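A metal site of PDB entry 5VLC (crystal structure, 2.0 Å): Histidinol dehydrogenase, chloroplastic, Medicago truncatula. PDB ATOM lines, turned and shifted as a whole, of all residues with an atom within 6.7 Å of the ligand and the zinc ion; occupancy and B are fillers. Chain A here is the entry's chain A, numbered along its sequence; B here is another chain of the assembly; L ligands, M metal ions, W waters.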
ATOM      1  N   VAL A 141     -10.335 -19.584 -28.911  1.00  0.00           N
ATOM      2  CA  VAL A 141     -11.213 -19.280 -27.813  1.00  0.00           C
ATOM      3  C   VAL A 141     -11.366 -17.756 -27.858  1.00  0.00           C
ATOM      4  O   VAL A 141     -10.428 -17.015 -27.506  1.00  0.00           O
ATOM      5  CB  VAL A 141     -10.582 -19.760 -26.485  1.00  0.00           C
ATOM      6  CG1 VAL A 141     -11.443 -19.356 -25.298  1.00  0.00           C
ATOM      7  CG2 VAL A 141     -10.335 -21.292 -26.503  1.00  0.00           C
ATOM      8  N   LEU A 142     -12.530 -17.264 -28.285  1.00  0.00           N
ATOM      9  CA  LEU A 142     -12.773 -15.807 -28.405  1.00  0.00           C
ATOM     10  C   LEU A 142     -14.043 -15.369 -27.740  1.00  0.00           C
ATOM     11  O   LEU A 142     -14.911 -14.759 -28.371  1.00  0.00           O
ATOM     12  CB  LEU A 142     -12.777 -15.387 -29.852  1.00  0.00           C
ATOM     13  CG  LEU A 142     -11.385 -15.424 -30.458  1.00  0.00           C
ATOM     14  CD1 LEU A 142     -11.516 -15.482 -31.968  1.00  0.00           C
ATOM     15  CD2 LEU A 142     -10.596 -14.188 -30.025  1.00  0.00           C
ATOM     16  N   SER A 144     -14.335 -12.982 -25.818  1.00  0.00           N
ATOM     17  CA  SER A 144     -14.385 -11.495 -25.859  1.00  0.00           C
ATOM     18  C   SER A 144     -15.212 -10.974 -27.020  1.00  0.00           C
ATOM     19  O   SER A 144     -16.076 -10.096 -26.867  1.00  0.00           O
ATOM     20  CB  SER A 144     -12.960 -10.868 -25.847  1.00  0.00           C
ATOM     21  OG  SER A 144     -12.158 -11.337 -26.951  1.00  0.00           O
ATOM     22  N   THR A 145     -14.955 -11.534 -28.207  1.00  0.00           N
ATOM     23  CA  THR A 145     -15.686 -11.178 -29.406  1.00  0.00           C
ATOM     24  C   THR A 145     -17.144 -11.535 -29.285  1.00  0.00           C
ATOM     25  O   THR A 145     -18.001 -10.795 -29.758  1.00  0.00           O
ATOM     26  CB  THR A 145     -15.077 -11.864 -30.631  1.00  0.00           C
ATOM     27  OG1 THR A 145     -13.665 -11.536 -30.714  1.00  0.00           O
ATOM     28  CG2 THR A 145     -15.781 -11.351 -31.946  1.00  0.00           C
ATOM     29  N   SER A 245      -5.515  -7.358 -37.321  1.00  0.00           N
ATOM     30  CA  SER A 245      -5.480  -6.339 -36.284  1.00  0.00           C
ATOM     31  C   SER A 245      -4.251  -5.400 -36.454  1.00  0.00           C
ATOM     32  O   SER A 245      -3.225  -5.763 -37.065  1.00  0.00           O
ATOM     33  CB  SER A 245      -5.487  -7.013 -34.940  1.00  0.00           C
ATOM     34  OG  SER A 245      -6.524  -7.970 -34.940  1.00  0.00           O
ATOM     35  N   GLU A 246      -4.400  -4.191 -35.912  1.00  0.00           N
ATOM     36  CA  GLU A 246      -3.447  -3.100 -36.063  1.00  0.00           C
ATOM     37  C   GLU A 246      -3.360  -2.306 -34.809  1.00  0.00           C
ATOM     38  O   GLU A 246      -4.366  -2.153 -34.110  1.00  0.00           O
ATOM     39  CB  GLU A 246      -3.948  -2.060 -37.067  1.00  0.00           C
ATOM     40  CG  GLU A 246      -4.371  -2.620 -38.357  1.00  0.00           C
ATOM     41  CD  GLU A 246      -4.941  -1.588 -39.317  1.00  0.00           C
ATOM     42  OE1 GLU A 246      -5.406  -0.462 -38.929  1.00  0.00           O
ATOM     43  OE2 GLU A 246      -4.904  -1.962 -40.502  1.00  0.00           O
ATOM     44  N   SER A 266       1.504  -6.563 -27.846  1.00  0.00           N
ATOM     45  CA  SER A 266       0.147  -7.041 -27.525  1.00  0.00           C
ATOM     46  C   SER A 266      -0.684  -7.379 -28.791  1.00  0.00           C
ATOM     47  O   SER A 266      -1.300  -8.426 -28.866  1.00  0.00           O
ATOM     48  CB  SER A 266      -0.583  -6.051 -26.592  1.00  0.00           C
ATOM     49  OG  SER A 266      -0.945  -4.862 -27.301  1.00  0.00           O
ATOM     50  N   GLN A 267      -0.691  -6.495 -29.781  1.00  0.00           N
ATOM     51  CA  GLN A 267      -1.392  -6.800 -31.064  1.00  0.00           C
ATOM     52  C   GLN A 267      -0.596  -7.523 -32.156  1.00  0.00           C
ATOM     53  O   GLN A 267      -1.185  -8.190 -33.022  1.00  0.00           O
ATOM     54  CB  GLN A 267      -2.077  -5.545 -31.595  1.00  0.00           C
ATOM     55  CG  GLN A 267      -2.927  -4.857 -30.510  1.00  0.00           C
ATOM     56  CD  GLN A 267      -3.866  -5.763 -29.671  1.00  0.00           C
ATOM     57  OE1 GLN A 267      -4.650  -6.545 -30.188  1.00  0.00           O
ATOM     58  NE2 GLN A 267      -3.771  -5.637 -28.344  1.00  0.00           N
ATOM     59  N   GLU A 269       1.147 -10.057 -31.698  1.00  0.00           N
ATOM     60  CA  GLU A 269       0.898 -11.504 -31.455  1.00  0.00           C
ATOM     61  C   GLU A 269      -0.379 -12.049 -32.073  1.00  0.00           C
ATOM     62  O   GLU A 269      -0.579 -13.276 -32.091  1.00  0.00           O
ATOM     63  CB  GLU A 269       0.981 -11.882 -29.964  1.00  0.00           C
ATOM     64  CG  GLU A 269      -0.252 -11.460 -29.131  1.00  0.00           C
ATOM     65  CD  GLU A 269      -0.336 -12.091 -27.755  1.00  0.00           C
ATOM     66  OE1 GLU A 269       0.521 -12.965 -27.415  1.00  0.00           O
ATOM     67  OE2 GLU A 269      -1.264 -11.703 -27.002  1.00  0.00           O
ATOM     68  N   HIS A 270      -1.271 -11.195 -32.581  1.00  0.00           N
ATOM     69  CA  HIS A 270      -2.504 -11.717 -33.166  1.00  0.00           C
ATOM     70  C   HIS A 270      -2.208 -12.635 -34.355  1.00  0.00           C
ATOM     71  O   HIS A 270      -2.928 -13.597 -34.589  1.00  0.00           O
ATOM     72  CB  HIS A 270      -3.480 -10.611 -33.563  1.00  0.00           C
ATOM     73  CG  HIS A 270      -4.406 -10.154 -32.471  1.00  0.00           C
ATOM     74  ND1 HIS A 270      -5.391 -10.957 -31.968  1.00  0.00           N
ATOM     75  CD2 HIS A 270      -4.503  -8.988 -31.811  1.00  0.00           C
ATOM     76  CE1 HIS A 270      -6.064 -10.311 -31.042  1.00  0.00           C
ATOM     77  NE2 HIS A 270      -5.541  -9.107 -30.923  1.00  0.00           N
ATOM     78  N   GLU A 335      -6.680   0.971 -36.819  1.00  0.00           N
ATOM     79  CA  GLU A 335      -7.729   0.331 -36.066  1.00  0.00           C
ATOM     80  C   GLU A 335      -7.745   0.786 -34.571  1.00  0.00           C
ATOM     81  O   GLU A 335      -8.806   1.126 -33.996  1.00  0.00           O
ATOM     82  CB  GLU A 335      -7.556  -1.180 -36.127  1.00  0.00           C
ATOM     83  CG  GLU A 335      -8.782  -1.947 -35.594  1.00  0.00           C
ATOM     84  CD  GLU A 335      -8.483  -3.408 -35.257  1.00  0.00           C
ATOM     85  OE1 GLU A 335      -7.273  -3.842 -35.189  1.00  0.00           O
ATOM     86  OE2 GLU A 335      -9.523  -4.141 -35.060  1.00  0.00           O
ATOM     87  N   HIS A 336      -6.572   0.782 -33.945  1.00  0.00           N
ATOM     88  CA  HIS A 336      -6.417   1.156 -32.553  1.00  0.00           C
ATOM     89  C   HIS A 336      -5.290   2.151 -32.483  1.00  0.00           C
ATOM     90  O   HIS A 336      -4.261   1.972 -33.157  1.00  0.00           O
ATOM     91  CB  HIS A 336      -5.957  -0.033 -31.683  1.00  0.00           C
ATOM     92  CG  HIS A 336      -6.910  -1.163 -31.671  1.00  0.00           C
ATOM     93  ND1 HIS A 336      -6.773  -2.246 -32.511  1.00  0.00           N
ATOM     94  CD2 HIS A 336      -8.021  -1.378 -30.932  1.00  0.00           C
ATOM     95  CE1 HIS A 336      -7.779  -3.094 -32.279  1.00  0.00           C
ATOM     96  NE2 HIS A 336      -8.535  -2.576 -31.318  1.00  0.00           N
ATOM     97  N   GLU A 365      -4.023  -1.181 -24.866  1.00  0.00           N
ATOM     98  CA  GLU A 365      -5.114  -1.600 -25.695  1.00  0.00           C
ATOM     99  C   GLU A 365      -5.847  -2.835 -25.133  1.00  0.00           C
ATOM    100  O   GLU A 365      -7.047  -2.971 -25.346  1.00  0.00           O
ATOM    101  CB  GLU A 365      -4.610  -1.908 -27.103  1.00  0.00           C
ATOM    102  CG  GLU A 365      -5.746  -2.512 -27.946  1.00  0.00           C
ATOM    103  CD  GLU A 365      -5.404  -2.831 -29.382  1.00  0.00           C
ATOM    104  OE1 GLU A 365      -4.477  -2.225 -29.990  1.00  0.00           O
ATOM    105  OE2 GLU A 365      -6.109  -3.718 -29.912  1.00  0.00           O
ATOM    106  N   SER A 366      -5.113  -3.718 -24.433  1.00  0.00           N
ATOM    107  CA  SER A 366      -5.684  -4.943 -23.844  1.00  0.00           C
ATOM    108  C   SER A 366      -6.928  -4.651 -23.091  1.00  0.00           C
ATOM    109  O   SER A 366      -7.886  -5.437 -23.156  1.00  0.00           O
ATOM    110  CB  SER A 366      -4.667  -5.677 -22.924  1.00  0.00           C
ATOM    111  OG  SER A 366      -3.460  -5.891 -23.593  1.00  0.00           O
ATOM    112  N   GLY A 368      -9.337  -2.417 -23.704  1.00  0.00           N
ATOM    113  CA  GLY A 368     -10.417  -2.290 -24.689  1.00  0.00           C
ATOM    114  C   GLY A 368     -10.743  -3.586 -25.404  1.00  0.00           C
ATOM    115  O   GLY A 368     -11.923  -3.874 -25.652  1.00  0.00           O
ATOM    116  N   ASP A 369      -9.693  -4.369 -25.720  1.00  0.00           N
ATOM    117  CA  ASP A 369      -9.863  -5.693 -26.273  1.00  0.00           C
ATOM    118  C   ASP A 369     -10.803  -6.558 -25.426  1.00  0.00           C
ATOM    119  O   ASP A 369     -11.517  -7.348 -26.013  1.00  0.00           O
ATOM    120  CB  ASP A 369      -8.532  -6.443 -26.475  1.00  0.00           C
ATOM    121  CG  ASP A 369      -7.688  -5.908 -27.651  1.00  0.00           C
ATOM    122  OD1 ASP A 369      -8.131  -4.948 -28.366  1.00  0.00           O
ATOM    123  OD2 ASP A 369      -6.585  -6.463 -27.870  1.00  0.00           O
ATOM    124  N   TYR A 370     -10.695  -6.413 -24.117  1.00  0.00           N
ATOM    125  CA  TYR A 370     -11.397  -7.228 -23.182  1.00  0.00           C
ATOM    126  C   TYR A 370     -12.536  -6.712 -22.310  1.00  0.00           C
ATOM    127  O   TYR A 370     -13.557  -7.303 -22.305  1.00  0.00           O
ATOM    128  CB  TYR A 370     -10.374  -7.927 -22.291  1.00  0.00           C
ATOM    129  CG  TYR A 370      -9.551  -8.931 -23.025  1.00  0.00           C
ATOM    130  CD1 TYR A 370     -10.115 -10.106 -23.424  1.00  0.00           C
ATOM    131  CD2 TYR A 370      -8.257  -8.680 -23.360  1.00  0.00           C
ATOM    132  CE1 TYR A 370      -9.391 -11.017 -24.116  1.00  0.00           C
ATOM    133  CE2 TYR A 370      -7.538  -9.589 -24.064  1.00  0.00           C
ATOM    134  CZ  TYR A 370      -8.115 -10.754 -24.441  1.00  0.00           C
ATOM    135  OH  TYR A 370      -7.464 -11.660 -25.124  1.00  0.00           O
ATOM    136  N   ASN A 375     -16.034  -1.302 -27.806  1.00  0.00           N
ATOM    137  CA  ASN A 375     -16.134  -2.438 -28.681  1.00  0.00           C
ATOM    138  C   ASN A 375     -14.878  -2.693 -29.479  1.00  0.00           C
ATOM    139  O   ASN A 375     -14.376  -1.788 -30.088  1.00  0.00           O
ATOM    140  CB  ASN A 375     -17.287  -2.222 -29.643  1.00  0.00           C
ATOM    141  CG  ASN A 375     -17.881  -3.528 -30.116  1.00  0.00           C
ATOM    142  OD1 ASN A 375     -17.213  -4.291 -30.835  1.00  0.00           O
ATOM    143  ND2 ASN A 375     -19.124  -3.791 -29.711  1.00  0.00           N
ATOM    144  N   HIS A 376     -14.361  -3.928 -29.465  1.00  0.00           N
ATOM    145  CA  HIS A 376     -13.126  -4.210 -30.157  1.00  0.00           C
ATOM    146  C   HIS A 376     -13.304  -4.622 -31.616  1.00  0.00           C
ATOM    147  O   HIS A 376     -12.320  -4.835 -32.300  1.00  0.00           O
ATOM    148  CB  HIS A 376     -12.256  -5.212 -29.387  1.00  0.00           C
ATOM    149  CG  HIS A 376     -12.638  -6.663 -29.524  1.00  0.00           C
ATOM    150  ND1 HIS A 376     -12.559  -7.524 -28.459  1.00  0.00           N
ATOM    151  CD2 HIS A 376     -13.073  -7.427 -30.565  1.00  0.00           C
ATOM    152  CE1 HIS A 376     -12.913  -8.732 -28.829  1.00  0.00           C
ATOM    153  NE2 HIS A 376     -13.230  -8.696 -30.111  1.00  0.00           N
ATOM    154  N   VAL A 377     -14.537  -4.753 -32.094  1.00  0.00           N
ATOM    155  CA  VAL A 377     -14.831  -5.081 -33.474  1.00  0.00           C
ATOM    156  C   VAL A 377     -14.778  -3.763 -34.280  1.00  0.00           C
ATOM    157  O   VAL A 377     -15.724  -2.970 -34.294  1.00  0.00           O
ATOM    158  CB  VAL A 377     -16.164  -5.820 -33.653  1.00  0.00           C
ATOM    159  CG1 VAL A 377     -16.307  -6.197 -35.152  1.00  0.00           C
ATOM    160  CG2 VAL A 377     -16.150  -7.102 -32.807  1.00  0.00           C
ATOM    161  N   LEU A 378     -13.640  -3.543 -34.928  1.00  0.00           N
ATOM    162  CA  LEU A 378     -13.263  -2.228 -35.388  1.00  0.00           C
ATOM    163  C   LEU A 378     -12.742  -2.243 -36.830  1.00  0.00           C
ATOM    164  O   LEU A 378     -12.288  -3.282 -37.306  1.00  0.00           O
ATOM    165  CB  LEU A 378     -12.198  -1.694 -34.442  1.00  0.00           C
ATOM    166  CG  LEU A 378     -12.700  -1.307 -33.067  1.00  0.00           C
ATOM    167  CD1 LEU A 378     -11.500  -1.316 -32.135  1.00  0.00           C
ATOM    168  CD2 LEU A 378     -13.345   0.022 -33.058  1.00  0.00           C
ATOM    169  N   GLU B 423      -7.857 -16.860 -23.530  1.00  0.00           N
ATOM    170  CA  GLU B 423      -7.805 -16.817 -24.997  1.00  0.00           C
ATOM    171  C   GLU B 423      -6.438 -17.224 -25.549  1.00  0.00           C
ATOM    172  O   GLU B 423      -6.292 -17.380 -26.742  1.00  0.00           O
ATOM    173  CB  GLU B 423      -8.160 -15.435 -25.542  1.00  0.00           C
ATOM    174  CG  GLU B 423      -9.582 -14.988 -25.169  1.00  0.00           C
ATOM    175  CD  GLU B 423     -10.054 -13.803 -26.019  1.00  0.00           C
ATOM    176  OE1 GLU B 423      -9.146 -13.074 -26.596  1.00  0.00           O
ATOM    177  OE2 GLU B 423     -11.321 -13.574 -26.108  1.00  0.00           O
ATOM    178  N   LEU B 425      -3.452 -15.500 -25.097  1.00  0.00           N
ATOM    179  CA  LEU B 425      -2.889 -14.253 -25.647  1.00  0.00           C
ATOM    180  C   LEU B 425      -2.052 -13.568 -24.594  1.00  0.00           C
ATOM    181  O   LEU B 425      -2.412 -12.547 -24.020  1.00  0.00           O
ATOM    182  CB  LEU B 425      -3.994 -13.381 -26.225  1.00  0.00           C
ATOM    183  CG  LEU B 425      -4.638 -13.904 -27.493  1.00  0.00           C
ATOM    184  CD1 LEU B 425      -5.702 -12.964 -28.006  1.00  0.00           C
ATOM    185  CD2 LEU B 425      -3.628 -14.111 -28.645  1.00  0.00           C
ATOM    186  N   HIS B 428      -1.090  -9.754 -24.739  1.00  0.00           N
ATOM    187  CA  HIS B 428      -2.198  -8.931 -24.213  1.00  0.00           C
ATOM    188  C   HIS B 428      -2.209  -8.888 -22.708  1.00  0.00           C
ATOM    189  O   HIS B 428      -2.414  -7.864 -22.099  1.00  0.00           O
ATOM    190  CB  HIS B 428      -3.562  -9.477 -24.670  1.00  0.00           C
ATOM    191  CG  HIS B 428      -3.920  -9.222 -26.091  1.00  0.00           C
ATOM    192  ND1 HIS B 428      -3.316  -9.844 -27.154  1.00  0.00           N
ATOM    193  CD2 HIS B 428      -4.865  -8.406 -26.630  1.00  0.00           C
ATOM    194  CE1 HIS B 428      -3.848  -9.422 -28.278  1.00  0.00           C
ATOM    195  NE2 HIS B 428      -4.798  -8.548 -27.988  1.00  0.00           N
HETATM  196  N1  LIG L   1      -7.345  -6.770 -30.769  1.00  0.00           N
HETATM  197  C1  LIG L   1      -8.524  -7.460 -31.415  1.00  0.00           C
HETATM  198  C2  LIG L   1      -9.482  -7.936 -30.375  1.00  0.00           C
HETATM  199  C3  LIG L   1      -8.963  -8.928 -29.401  1.00  0.00           C
HETATM  200  N2  LIG L   1      -7.746  -8.934 -28.802  1.00  0.00           N
HETATM  201  C4  LIG L   1      -9.555 -10.063 -28.873  1.00  0.00           C
HETATM  202  C5  LIG L   1      -7.629  -9.981 -27.973  1.00  0.00           C
HETATM  203  N3  LIG L   1      -8.742 -10.702 -28.007  1.00  0.00           N
HETATM  204  C6  LIG L   1      -9.232  -6.521 -32.466  1.00  0.00           C
HETATM  205  O1  LIG L   1      -9.832  -5.435 -31.780  1.00  0.00           O
HETATM  206 ZN    ZN M   1      -6.137  -7.742 -29.397  1.00  0.00          ZN
HETATM  207  O   HOH W   1      -9.076  -6.920 -35.687  1.00  0.00           O
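Of the 24 residues printed, 4 come within 4 Å of the zinc ion.
The backbone carbonyl oxygen of Asp 369 is in hydrogen-bond range of a ring nitrogen (ND1) of His 376, 2.7 Å away. The side-chain amide nitrogen of Gln 267 sits close to the side-chain carboxylate of Glu 365 (3.4 Å). ND1 of His 428 of chain B lies close to O of Ser 266, 3.0 Å away. NE2 of His 376 sits at hydrogen-bond distance from OG1 of Thr 145 (2.9 Å). A ring nitrogen (NE2) of His 336 sits close to the side-chain carboxylate (OE2) of Glu 365, at 3.0 Å. OE1 of Glu 335 lies close to ND1 of His 336 (3.2 Å). ND1 of His 336 lies within hydrogen-bond range of O of Glu 246 (2.9 Å). The side-chain carboxylate of Glu 246 lies within hydrogen-bond range of the backbone NH of Glu 335 (2.9 Å).
O of His 376 lies within hydrogen-bond range of O1 of the ligand. The side-chain carboxylate of Glu 423 of chain B is in hydrogen-bond range of a nitrogen (N3) of the ligand (2.8 Å). An oxygen (O1) of the ligand sits close to a ring nitrogen (NE2) of His 336 (3.2 Å). A nitrogen (N3) of the ligand is in hydrogen-bond range of the side-chain hydroxyl (OH) of Tyr 370 (3.3 Å). N1 of the ligand sits close to OE2 of Glu 365, 3.4 Å away.
OD2 of Asp 369 binds the zinc ion (2.0 Å). OE1 of Gln 267 is bound to the zinc ion (2.1 Å). The zinc ion is bound by a nitrogen (N1) of the ligand (2.1 Å). N2 of the ligand is bound to the zinc ion, 2.1 Å away. The zinc ion is bound by NE2 of His 428 of chain B (2.1 Å). NE2 of His 270 is bound to the zinc ion (2.1 Å).
Water W1 bridges OG of Ser 245 and OE2 of Glu 335.
Merely in contact with the ligand: Ser 144, Ser 245, Glu 335 and Leu 425 of chain B. 13 residues have an atom within 4 Å of the ligand: Ser 144, Ser 245, Gln 267, His 270, Glu 335, His 336, Glu 365, Asp 369, Tyr 370, His 376, Glu 423 of chain B, Leu 425 of chain B and His 428 of chain B. Along chain A the residues within 4 Å of the ligand span positions 144 to 376. The nearest printed residue that does not touch the ligand is Leu 142 (4.4 Å).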
